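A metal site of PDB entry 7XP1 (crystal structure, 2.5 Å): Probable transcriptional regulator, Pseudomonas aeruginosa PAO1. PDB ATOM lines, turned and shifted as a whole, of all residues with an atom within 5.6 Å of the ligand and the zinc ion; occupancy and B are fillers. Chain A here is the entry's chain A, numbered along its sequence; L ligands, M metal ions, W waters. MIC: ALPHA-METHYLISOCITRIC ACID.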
ATOM      1  N   TYR A  78     -22.022   5.117  17.553  1.00  0.00           N
ATOM      2  CA  TYR A  78     -23.103   5.597  16.694  1.00  0.00           C
ATOM      3  C   TYR A  78     -23.010   7.100  16.437  1.00  0.00           C
ATOM      4  O   TYR A  78     -23.552   7.575  15.433  1.00  0.00           O
ATOM      5  CB  TYR A  78     -24.450   5.252  17.314  1.00  0.00           C
ATOM      6  CG  TYR A  78     -24.975   3.916  16.843  1.00  0.00           C
ATOM      7  CD1 TYR A  78     -24.516   2.730  17.392  1.00  0.00           C
ATOM      8  CD2 TYR A  78     -25.925   3.845  15.826  1.00  0.00           C
ATOM      9  CE1 TYR A  78     -24.981   1.503  16.961  1.00  0.00           C
ATOM     10  CE2 TYR A  78     -26.402   2.617  15.376  1.00  0.00           C
ATOM     11  CZ  TYR A  78     -25.919   1.458  15.953  1.00  0.00           C
ATOM     12  OH  TYR A  78     -26.393   0.234  15.512  1.00  0.00           O
ATOM     13  N   ARG A  81     -20.760   7.182  13.450  1.00  0.00           N
ATOM     14  CA  ARG A  81     -21.486   6.600  12.333  1.00  0.00           C
ATOM     15  C   ARG A  81     -22.542   7.550  11.796  1.00  0.00           C
ATOM     16  O   ARG A  81     -22.784   7.596  10.580  1.00  0.00           O
ATOM     17  CB  ARG A  81     -22.122   5.273  12.747  1.00  0.00           C
ATOM     18  CG  ARG A  81     -22.839   4.570  11.608  1.00  0.00           C
ATOM     19  CD  ARG A  81     -23.570   3.323  12.086  1.00  0.00           C
ATOM     20  NE  ARG A  81     -24.283   2.697  10.971  1.00  0.00           N
ATOM     21  CZ  ARG A  81     -25.352   1.920  11.110  1.00  0.00           C
ATOM     22  NH1 ARG A  81     -25.850   1.633  12.303  1.00  0.00           N
ATOM     23  NH2 ARG A  81     -25.940   1.439  10.024  1.00  0.00           N
ATOM     24  N   GLN A 126     -31.348 -10.715  13.234  1.00  0.00           N
ATOM     25  CA  GLN A 126     -31.768 -10.155  11.960  1.00  0.00           C
ATOM     26  C   GLN A 126     -30.578 -10.100  11.010  1.00  0.00           C
ATOM     27  O   GLN A 126     -29.442  -9.862  11.439  1.00  0.00           O
ATOM     28  CB  GLN A 126     -32.378  -8.759  12.131  1.00  0.00           C
ATOM     29  CG  GLN A 126     -33.204  -8.304  10.950  1.00  0.00           C
ATOM     30  CD  GLN A 126     -32.874  -6.891  10.503  1.00  0.00           C
ATOM     31  OE1 GLN A 126     -32.123  -6.180  11.174  1.00  0.00           O
ATOM     32  NE2 GLN A 126     -33.407  -6.492   9.358  1.00  0.00           N
ATOM     33  N   GLU A 127     -30.853 -10.308   9.725  1.00  0.00           N
ATOM     34  CA  GLU A 127     -29.781 -10.306   8.729  1.00  0.00           C
ATOM     35  C   GLU A 127     -29.257  -8.892   8.481  1.00  0.00           C
ATOM     36  O   GLU A 127     -28.054  -8.645   8.564  1.00  0.00           O
ATOM     37  CB  GLU A 127     -30.284 -10.935   7.420  1.00  0.00           C
ATOM     38  CG  GLU A 127     -31.583 -10.365   6.846  1.00  0.00           C
ATOM     39  CD  GLU A 127     -32.835 -10.893   7.532  1.00  0.00           C
ATOM     40  OE1 GLU A 127     -32.912 -10.847   8.772  1.00  0.00           O
ATOM     41  OE2 GLU A 127     -33.747 -11.357   6.813  1.00  0.00           O
ATOM     42  N   GLY A 128     -30.149  -7.952   8.199  1.00  0.00           N
ATOM     43  CA  GLY A 128     -29.781  -6.567   7.975  1.00  0.00           C
ATOM     44  C   GLY A 128     -29.572  -6.256   6.501  1.00  0.00           C
ATOM     45  O   GLY A 128     -29.526  -7.130   5.637  1.00  0.00           O
ATOM     46  N   ASP A 129     -29.457  -4.961   6.230  1.00  0.00           N
ATOM     47  CA  ASP A 129     -29.280  -4.472   4.874  1.00  0.00           C
ATOM     48  C   ASP A 129     -27.948  -3.757   4.715  1.00  0.00           C
ATOM     49  O   ASP A 129     -27.896  -2.598   4.293  1.00  0.00           O
ATOM     50  CB  ASP A 129     -30.426  -3.542   4.494  1.00  0.00           C
ATOM     51  CG  ASP A 129     -30.865  -3.718   3.055  1.00  0.00           C
ATOM     52  OD1 ASP A 129     -29.993  -3.979   2.188  1.00  0.00           O
ATOM     53  OD2 ASP A 129     -32.078  -3.576   2.779  1.00  0.00           O
ATOM     54  N   TYR A 130     -26.852  -4.442   5.049  1.00  0.00           N
ATOM     55  CA  TYR A 130     -25.525  -3.848   4.894  1.00  0.00           C
ATOM     56  C   TYR A 130     -25.239  -3.469   3.449  1.00  0.00           C
ATOM     57  O   TYR A 130     -24.514  -2.509   3.195  1.00  0.00           O
ATOM     58  CB  TYR A 130     -24.452  -4.796   5.414  1.00  0.00           C
ATOM     59  CG  TYR A 130     -23.038  -4.322   5.147  1.00  0.00           C
ATOM     60  CD1 TYR A 130     -22.600  -3.102   5.644  1.00  0.00           C
ATOM     61  CD2 TYR A 130     -22.162  -5.085   4.396  1.00  0.00           C
ATOM     62  CE1 TYR A 130     -21.313  -2.655   5.403  1.00  0.00           C
ATOM     63  CE2 TYR A 130     -20.870  -4.648   4.146  1.00  0.00           C
ATOM     64  CZ  TYR A 130     -20.453  -3.433   4.651  1.00  0.00           C
ATOM     65  OH  TYR A 130     -19.177  -3.000   4.396  1.00  0.00           O
ATOM     66  N   PHE A 132     -27.291  -2.133   1.307  1.00  0.00           N
ATOM     67  CA  PHE A 132     -27.840  -0.796   1.071  1.00  0.00           C
ATOM     68  C   PHE A 132     -26.876   0.286   1.534  1.00  0.00           C
ATOM     69  O   PHE A 132     -26.536   1.194   0.769  1.00  0.00           O
ATOM     70  CB  PHE A 132     -29.194  -0.654   1.782  1.00  0.00           C
ATOM     71  CG  PHE A 132     -29.892   0.642   1.494  1.00  0.00           C
ATOM     72  CD1 PHE A 132     -30.459   0.883   0.254  1.00  0.00           C
ATOM     73  CD2 PHE A 132     -29.981   1.625   2.473  1.00  0.00           C
ATOM     74  CE1 PHE A 132     -31.104   2.076  -0.010  1.00  0.00           C
ATOM     75  CE2 PHE A 132     -30.617   2.828   2.214  1.00  0.00           C
ATOM     76  CZ  PHE A 132     -31.179   3.045   0.970  1.00  0.00           C
ATOM     77  N   HIS A 133     -26.420   0.204   2.789  1.00  0.00           N
ATOM     78  CA  HIS A 133     -25.483   1.192   3.308  1.00  0.00           C
ATOM     79  C   HIS A 133     -24.173   1.157   2.546  1.00  0.00           C
ATOM     80  O   HIS A 133     -23.548   2.202   2.311  1.00  0.00           O
ATOM     81  CB  HIS A 133     -25.250   0.961   4.798  1.00  0.00           C
ATOM     82  CG  HIS A 133     -26.414   1.309   5.651  1.00  0.00           C
ATOM     83  ND1 HIS A 133     -26.341   2.233   6.672  1.00  0.00           N
ATOM     84  CD2 HIS A 133     -27.693   0.865   5.656  1.00  0.00           C
ATOM     85  CE1 HIS A 133     -27.517   2.346   7.264  1.00  0.00           C
ATOM     86  NE2 HIS A 133     -28.360   1.518   6.655  1.00  0.00           N
ATOM     87  N   TYR A 154     -17.771  -0.529  11.222  1.00  0.00           N
ATOM     88  CA  TYR A 154     -18.804  -1.530  11.003  1.00  0.00           C
ATOM     89  C   TYR A 154     -18.502  -2.865  11.679  1.00  0.00           C
ATOM     90  O   TYR A 154     -19.404  -3.686  11.819  1.00  0.00           O
ATOM     91  CB  TYR A 154     -19.033  -1.740   9.505  1.00  0.00           C
ATOM     92  CG  TYR A 154     -20.265  -1.038   8.994  1.00  0.00           C
ATOM     93  CD1 TYR A 154     -21.521  -1.589   9.155  1.00  0.00           C
ATOM     94  CD2 TYR A 154     -20.171   0.203   8.360  1.00  0.00           C
ATOM     95  CE1 TYR A 154     -22.654  -0.953   8.696  1.00  0.00           C
ATOM     96  CE2 TYR A 154     -21.302   0.856   7.905  1.00  0.00           C
ATOM     97  CZ  TYR A 154     -22.543   0.278   8.073  1.00  0.00           C
ATOM     98  OH  TYR A 154     -23.673   0.917   7.623  1.00  0.00           O
ATOM     99  N   VAL A 157     -19.829  -2.180  15.119  1.00  0.00           N
ATOM    100  CA  VAL A 157     -21.276  -2.094  14.967  1.00  0.00           C
ATOM    101  C   VAL A 157     -21.892  -3.494  14.981  1.00  0.00           C
ATOM    102  O   VAL A 157     -22.891  -3.736  15.670  1.00  0.00           O
ATOM    103  CB  VAL A 157     -21.629  -1.355  13.659  1.00  0.00           C
ATOM    104  CG1 VAL A 157     -23.048  -1.666  13.230  1.00  0.00           C
ATOM    105  CG2 VAL A 157     -21.436   0.144  13.820  1.00  0.00           C
ATOM    106  N   ARG A 161     -25.075  -5.439  17.211  1.00  0.00           N
ATOM    107  CA  ARG A 161     -26.275  -6.043  16.620  1.00  0.00           C
ATOM    108  C   ARG A 161     -26.307  -7.549  16.781  1.00  0.00           C
ATOM    109  O   ARG A 161     -27.391  -8.145  16.721  1.00  0.00           O
ATOM    110  CB  ARG A 161     -26.358  -5.672  15.142  1.00  0.00           C
ATOM    111  CG  ARG A 161     -27.125  -4.389  14.868  1.00  0.00           C
ATOM    112  CD  ARG A 161     -28.303  -4.671  13.945  1.00  0.00           C
ATOM    113  NE  ARG A 161     -27.841  -5.061  12.626  1.00  0.00           N
ATOM    114  CZ  ARG A 161     -28.560  -5.730  11.740  1.00  0.00           C
ATOM    115  NH1 ARG A 161     -29.810  -6.095  11.994  1.00  0.00           N
ATOM    116  NH2 ARG A 161     -28.023  -6.046  10.570  1.00  0.00           N
ATOM    117  N   THR A 166     -32.647  -7.264  17.214  1.00  0.00           N
ATOM    118  CA  THR A 166     -33.627  -6.206  17.013  1.00  0.00           C
ATOM    119  C   THR A 166     -35.019  -6.686  17.443  1.00  0.00           C
ATOM    120  O   THR A 166     -35.253  -7.876  17.686  1.00  0.00           O
ATOM    121  CB  THR A 166     -33.655  -5.764  15.558  1.00  0.00           C
ATOM    122  OG1 THR A 166     -33.725  -6.912  14.702  1.00  0.00           O
ATOM    123  CG2 THR A 166     -32.385  -4.985  15.215  1.00  0.00           C
ATOM    124  N   ARG A 170     -38.592  -3.934  13.885  1.00  0.00           N
ATOM    125  CA  ARG A 170     -37.439  -3.140  13.459  1.00  0.00           C
ATOM    126  C   ARG A 170     -37.067  -3.420  12.000  1.00  0.00           C
ATOM    127  O   ARG A 170     -36.766  -2.463  11.271  1.00  0.00           O
ATOM    128  CB  ARG A 170     -36.246  -3.387  14.383  1.00  0.00           C
ATOM    129  CG  ARG A 170     -35.059  -2.472  14.111  1.00  0.00           C
ATOM    130  CD  ARG A 170     -35.506  -1.013  14.086  1.00  0.00           C
ATOM    131  NE  ARG A 170     -34.520  -0.151  13.438  1.00  0.00           N
ATOM    132  CZ  ARG A 170     -34.792   1.044  12.952  1.00  0.00           C
ATOM    133  NH1 ARG A 170     -36.013   1.550  13.004  1.00  0.00           N
ATOM    134  NH2 ARG A 170     -33.820   1.756  12.389  1.00  0.00           N
ATOM    135  N   ALA A 174     -36.952  -0.261   9.367  1.00  0.00           N
ATOM    136  CA  ALA A 174     -35.727   0.155   8.688  1.00  0.00           C
ATOM    137  C   ALA A 174     -35.875   0.141   7.180  1.00  0.00           C
ATOM    138  O   ALA A 174     -35.220   0.934   6.489  1.00  0.00           O
ATOM    139  CB  ALA A 174     -34.558  -0.747   9.118  1.00  0.00           C
ATOM    140  N   HIS A 178     -35.051   3.146   4.809  1.00  0.00           N
ATOM    141  CA  HIS A 178     -34.132   2.981   3.690  1.00  0.00           C
ATOM    142  C   HIS A 178     -34.714   3.575   2.406  1.00  0.00           C
ATOM    143  O   HIS A 178     -33.995   4.225   1.630  1.00  0.00           O
ATOM    144  CB  HIS A 178     -33.803   1.511   3.498  1.00  0.00           C
ATOM    145  CG  HIS A 178     -32.821   0.969   4.488  1.00  0.00           C
ATOM    146  ND1 HIS A 178     -32.702  -0.373   4.765  1.00  0.00           N
ATOM    147  CD2 HIS A 178     -31.924   1.597   5.282  1.00  0.00           C
ATOM    148  CE1 HIS A 178     -31.764  -0.551   5.682  1.00  0.00           C
ATOM    149  NE2 HIS A 178     -31.278   0.632   6.013  1.00  0.00           N
ATOM    150  N   HIS A 200     -32.251   7.612  10.692  1.00  0.00           N
ATOM    151  CA  HIS A 200     -32.251   6.161  10.634  1.00  0.00           C
ATOM    152  C   HIS A 200     -31.136   5.573  11.503  1.00  0.00           C
ATOM    153  O   HIS A 200     -31.314   4.515  12.112  1.00  0.00           O
ATOM    154  CB  HIS A 200     -32.115   5.685   9.188  1.00  0.00           C
ATOM    155  CG  HIS A 200     -31.763   4.242   9.045  1.00  0.00           C
ATOM    156  ND1 HIS A 200     -32.648   3.225   9.346  1.00  0.00           N
ATOM    157  CD2 HIS A 200     -30.615   3.632   8.644  1.00  0.00           C
ATOM    158  CE1 HIS A 200     -32.060   2.059   9.126  1.00  0.00           C
ATOM    159  NE2 HIS A 200     -30.835   2.282   8.700  1.00  0.00           N
ATOM    160  N   ILE A 201     -29.979   6.242  11.547  1.00  0.00           N
ATOM    161  CA  ILE A 201     -28.909   5.809  12.435  1.00  0.00           C
ATOM    162  C   ILE A 201     -29.341   5.955  13.885  1.00  0.00           C
ATOM    163  O   ILE A 201     -29.104   5.069  14.717  1.00  0.00           O
ATOM    164  CB  ILE A 201     -27.617   6.585  12.142  1.00  0.00           C
ATOM    165  CG1 ILE A 201     -27.147   6.351  10.714  1.00  0.00           C
ATOM    166  CG2 ILE A 201     -26.519   6.204  13.124  1.00  0.00           C
ATOM    167  CD1 ILE A 201     -26.847   4.912  10.408  1.00  0.00           C
ATOM    168  N   ALA A 203     -32.407   5.906  15.008  1.00  0.00           N
ATOM    169  CA  ALA A 203     -33.407   4.883  15.289  1.00  0.00           C
ATOM    170  C   ALA A 203     -32.739   3.542  15.559  1.00  0.00           C
ATOM    171  O   ALA A 203     -33.222   2.766  16.393  1.00  0.00           O
ATOM    172  CB  ALA A 203     -34.379   4.774  14.115  1.00  0.00           C
ATOM    173  N   SER A 204     -31.634   3.262  14.875  1.00  0.00           N
ATOM    174  CA  SER A 204     -30.908   2.021  15.122  1.00  0.00           C
ATOM    175  C   SER A 204     -30.307   2.000  16.522  1.00  0.00           C
ATOM    176  O   SER A 204     -30.340   0.968  17.201  1.00  0.00           O
ATOM    177  CB  SER A 204     -29.821   1.833  14.063  1.00  0.00           C
ATOM    178  OG  SER A 204     -29.133   0.605  14.249  1.00  0.00           O
ATOM    179  N   ASN A 207     -32.961   1.415  19.124  1.00  0.00           N
ATOM    180  CA  ASN A 207     -33.397   0.021  19.072  1.00  0.00           C
ATOM    181  C   ASN A 207     -32.452  -0.876  19.866  1.00  0.00           C
ATOM    182  O   ASN A 207     -32.887  -1.802  20.555  1.00  0.00           O
ATOM    183  CB  ASN A 207     -33.475  -0.445  17.618  1.00  0.00           C
ATOM    184  CG  ASN A 207     -33.979  -1.858  17.482  1.00  0.00           C
ATOM    185  OD1 ASN A 207     -33.207  -2.792  17.273  1.00  0.00           O
ATOM    186  ND2 ASN A 207     -35.292  -2.027  17.601  1.00  0.00           N
ATOM    187  N   ILE A 208     -31.144  -0.608  19.788  1.00  0.00           N
ATOM    188  CA  ILE A 208     -30.176  -1.384  20.561  1.00  0.00           C
ATOM    189  C   ILE A 208     -30.231  -0.994  22.028  1.00  0.00           C
ATOM    190  O   ILE A 208     -30.100  -1.840  22.920  1.00  0.00           O
ATOM    191  CB  ILE A 208     -28.765  -1.214  19.969  1.00  0.00           C
ATOM    192  CG1 ILE A 208     -28.603  -2.063  18.716  1.00  0.00           C
ATOM    193  CG2 ILE A 208     -27.696  -1.579  20.998  1.00  0.00           C
ATOM    194  CD1 ILE A 208     -27.368  -1.748  17.907  1.00  0.00           C
HETATM  195  C1  MIC L   1     -29.337  -2.454   8.423  1.00  0.00           C
HETATM  196  O1  MIC L   1     -28.718  -3.520   8.645  1.00  0.00           O
HETATM  197  O2  MIC L   1     -29.085  -1.712   7.448  1.00  0.00           O
HETATM  198  C2  MIC L   1     -30.453  -2.048   9.362  1.00  0.00           C
HETATM  199  CM2 MIC L   1     -31.405  -3.222   9.498  1.00  0.00           C
HETATM  200  O7  MIC L   1     -31.174  -0.944   8.810  1.00  0.00           O
HETATM  201  C3  MIC L   1     -29.953  -1.644  10.759  1.00  0.00           C
HETATM  202  C4  MIC L   1     -31.100  -0.986  11.509  1.00  0.00           C
HETATM  203  C5  MIC L   1     -31.101  -1.387  12.956  1.00  0.00           C
HETATM  204  O3  MIC L   1     -30.219  -2.183  13.363  1.00  0.00           O
HETATM  205  O4  MIC L   1     -31.971  -0.906  13.704  1.00  0.00           O
HETATM  206  C6  MIC L   1     -28.767  -0.707  10.747  1.00  0.00           C
HETATM  207  O5  MIC L   1     -28.021  -0.687  11.754  1.00  0.00           O
HETATM  208  O6  MIC L   1     -28.569   0.037   9.764  1.00  0.00           O
HETATM  209 ZN    ZN M   1     -29.928   0.340   7.843  1.00  0.00          ZN
HETATM  210  O   HOH W   1     -30.128  -2.318  15.792  1.00  0.00           O
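An oxygen (O4) of the ligand lies within salt-bridge range of the guanidinium group (NE) of Arg 170, 2.7 Å away.
The backbone NH (N) of Asp 129 sits at hydrogen-bond distance from an oxygen (O1) of the ligand (2.9 Å).
An oxygen (O5) of the ligand is in salt-bridge range of the guanidinium group (NH1) of Arg 81, at 3.2 Å.
The side-chain hydroxyl (OG) of Ser 204 lies within hydrogen-bond range of an oxygen (O5) of the ligand (3.0 Å).
The guanidinium group (NH2) of Arg 161 lies within salt-bridge range of an oxygen (O1) of the ligand (3.3 Å).
A ring nitrogen (ND1) of His 178 lies close to the backbone carbonyl oxygen (O) of Ala 174, at 3.3 Å.
A ring nitrogen (ND1) of His 133 lies close to the guanidinium group (NH2) of Arg 81 (3.5 Å).
A ring nitrogen (ND1) of His 133 sits at hydrogen-bond distance from the side-chain hydroxyl of Tyr 154, at 3.1 Å.
OD1 of Asp 129 lies within hydrogen-bond range of N of Phe 132.
NH2 of Arg 81 sits at hydrogen-bond distance from OH of Tyr 154 (3.3 Å).
The side-chain hydroxyl of Ser 204 sits at hydrogen-bond distance from the side-chain hydroxyl of Tyr 78 (3.0 Å).
The side-chain amide oxygen (OE1) of Gln 126 sits at hydrogen-bond distance from the guanidinium group (NH1) of Arg 161.
NH2 of Arg 161 lies within hydrogen-bond range of O of Glu 127, at 3.3 Å.
OE1 of Gln 126 touches CM2 of the ligand, at 3.5 Å.
Gly 128 touches the ligand.
Thr 166 touches the ligand.
CB of Ala 174 touches O7 of the ligand, at 3.4 Å.
Within 4 Å of the ligand: Arg 81, Gln 126, Gly 128, Asp 129, His 133, Arg 161, Thr 166, Arg 170, Ala 174, His 178, His 200 and Ser 204.
The zinc ion is bound by O7 of the ligand, at 2.0 Å.
The zinc ion is bound by O2 of the ligand (2.3 Å).
The zinc ion is bound by NE2 of His 178.
A ring nitrogen (NE2) of His 133 is bound to the zinc ion, at 2.3 Å.
The zinc ion is bound by a ring nitrogen (NE2) of His 200 (2.3 Å).
An oxygen (O6) of the ligand binds the zinc ion (2.4 Å).
The zinc ion has six donor atoms within binding distance.
Water W1 lies within hydrogen-bond range of O3 of the ligand, OD1 of Asn 207 and OG of Ser 204.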
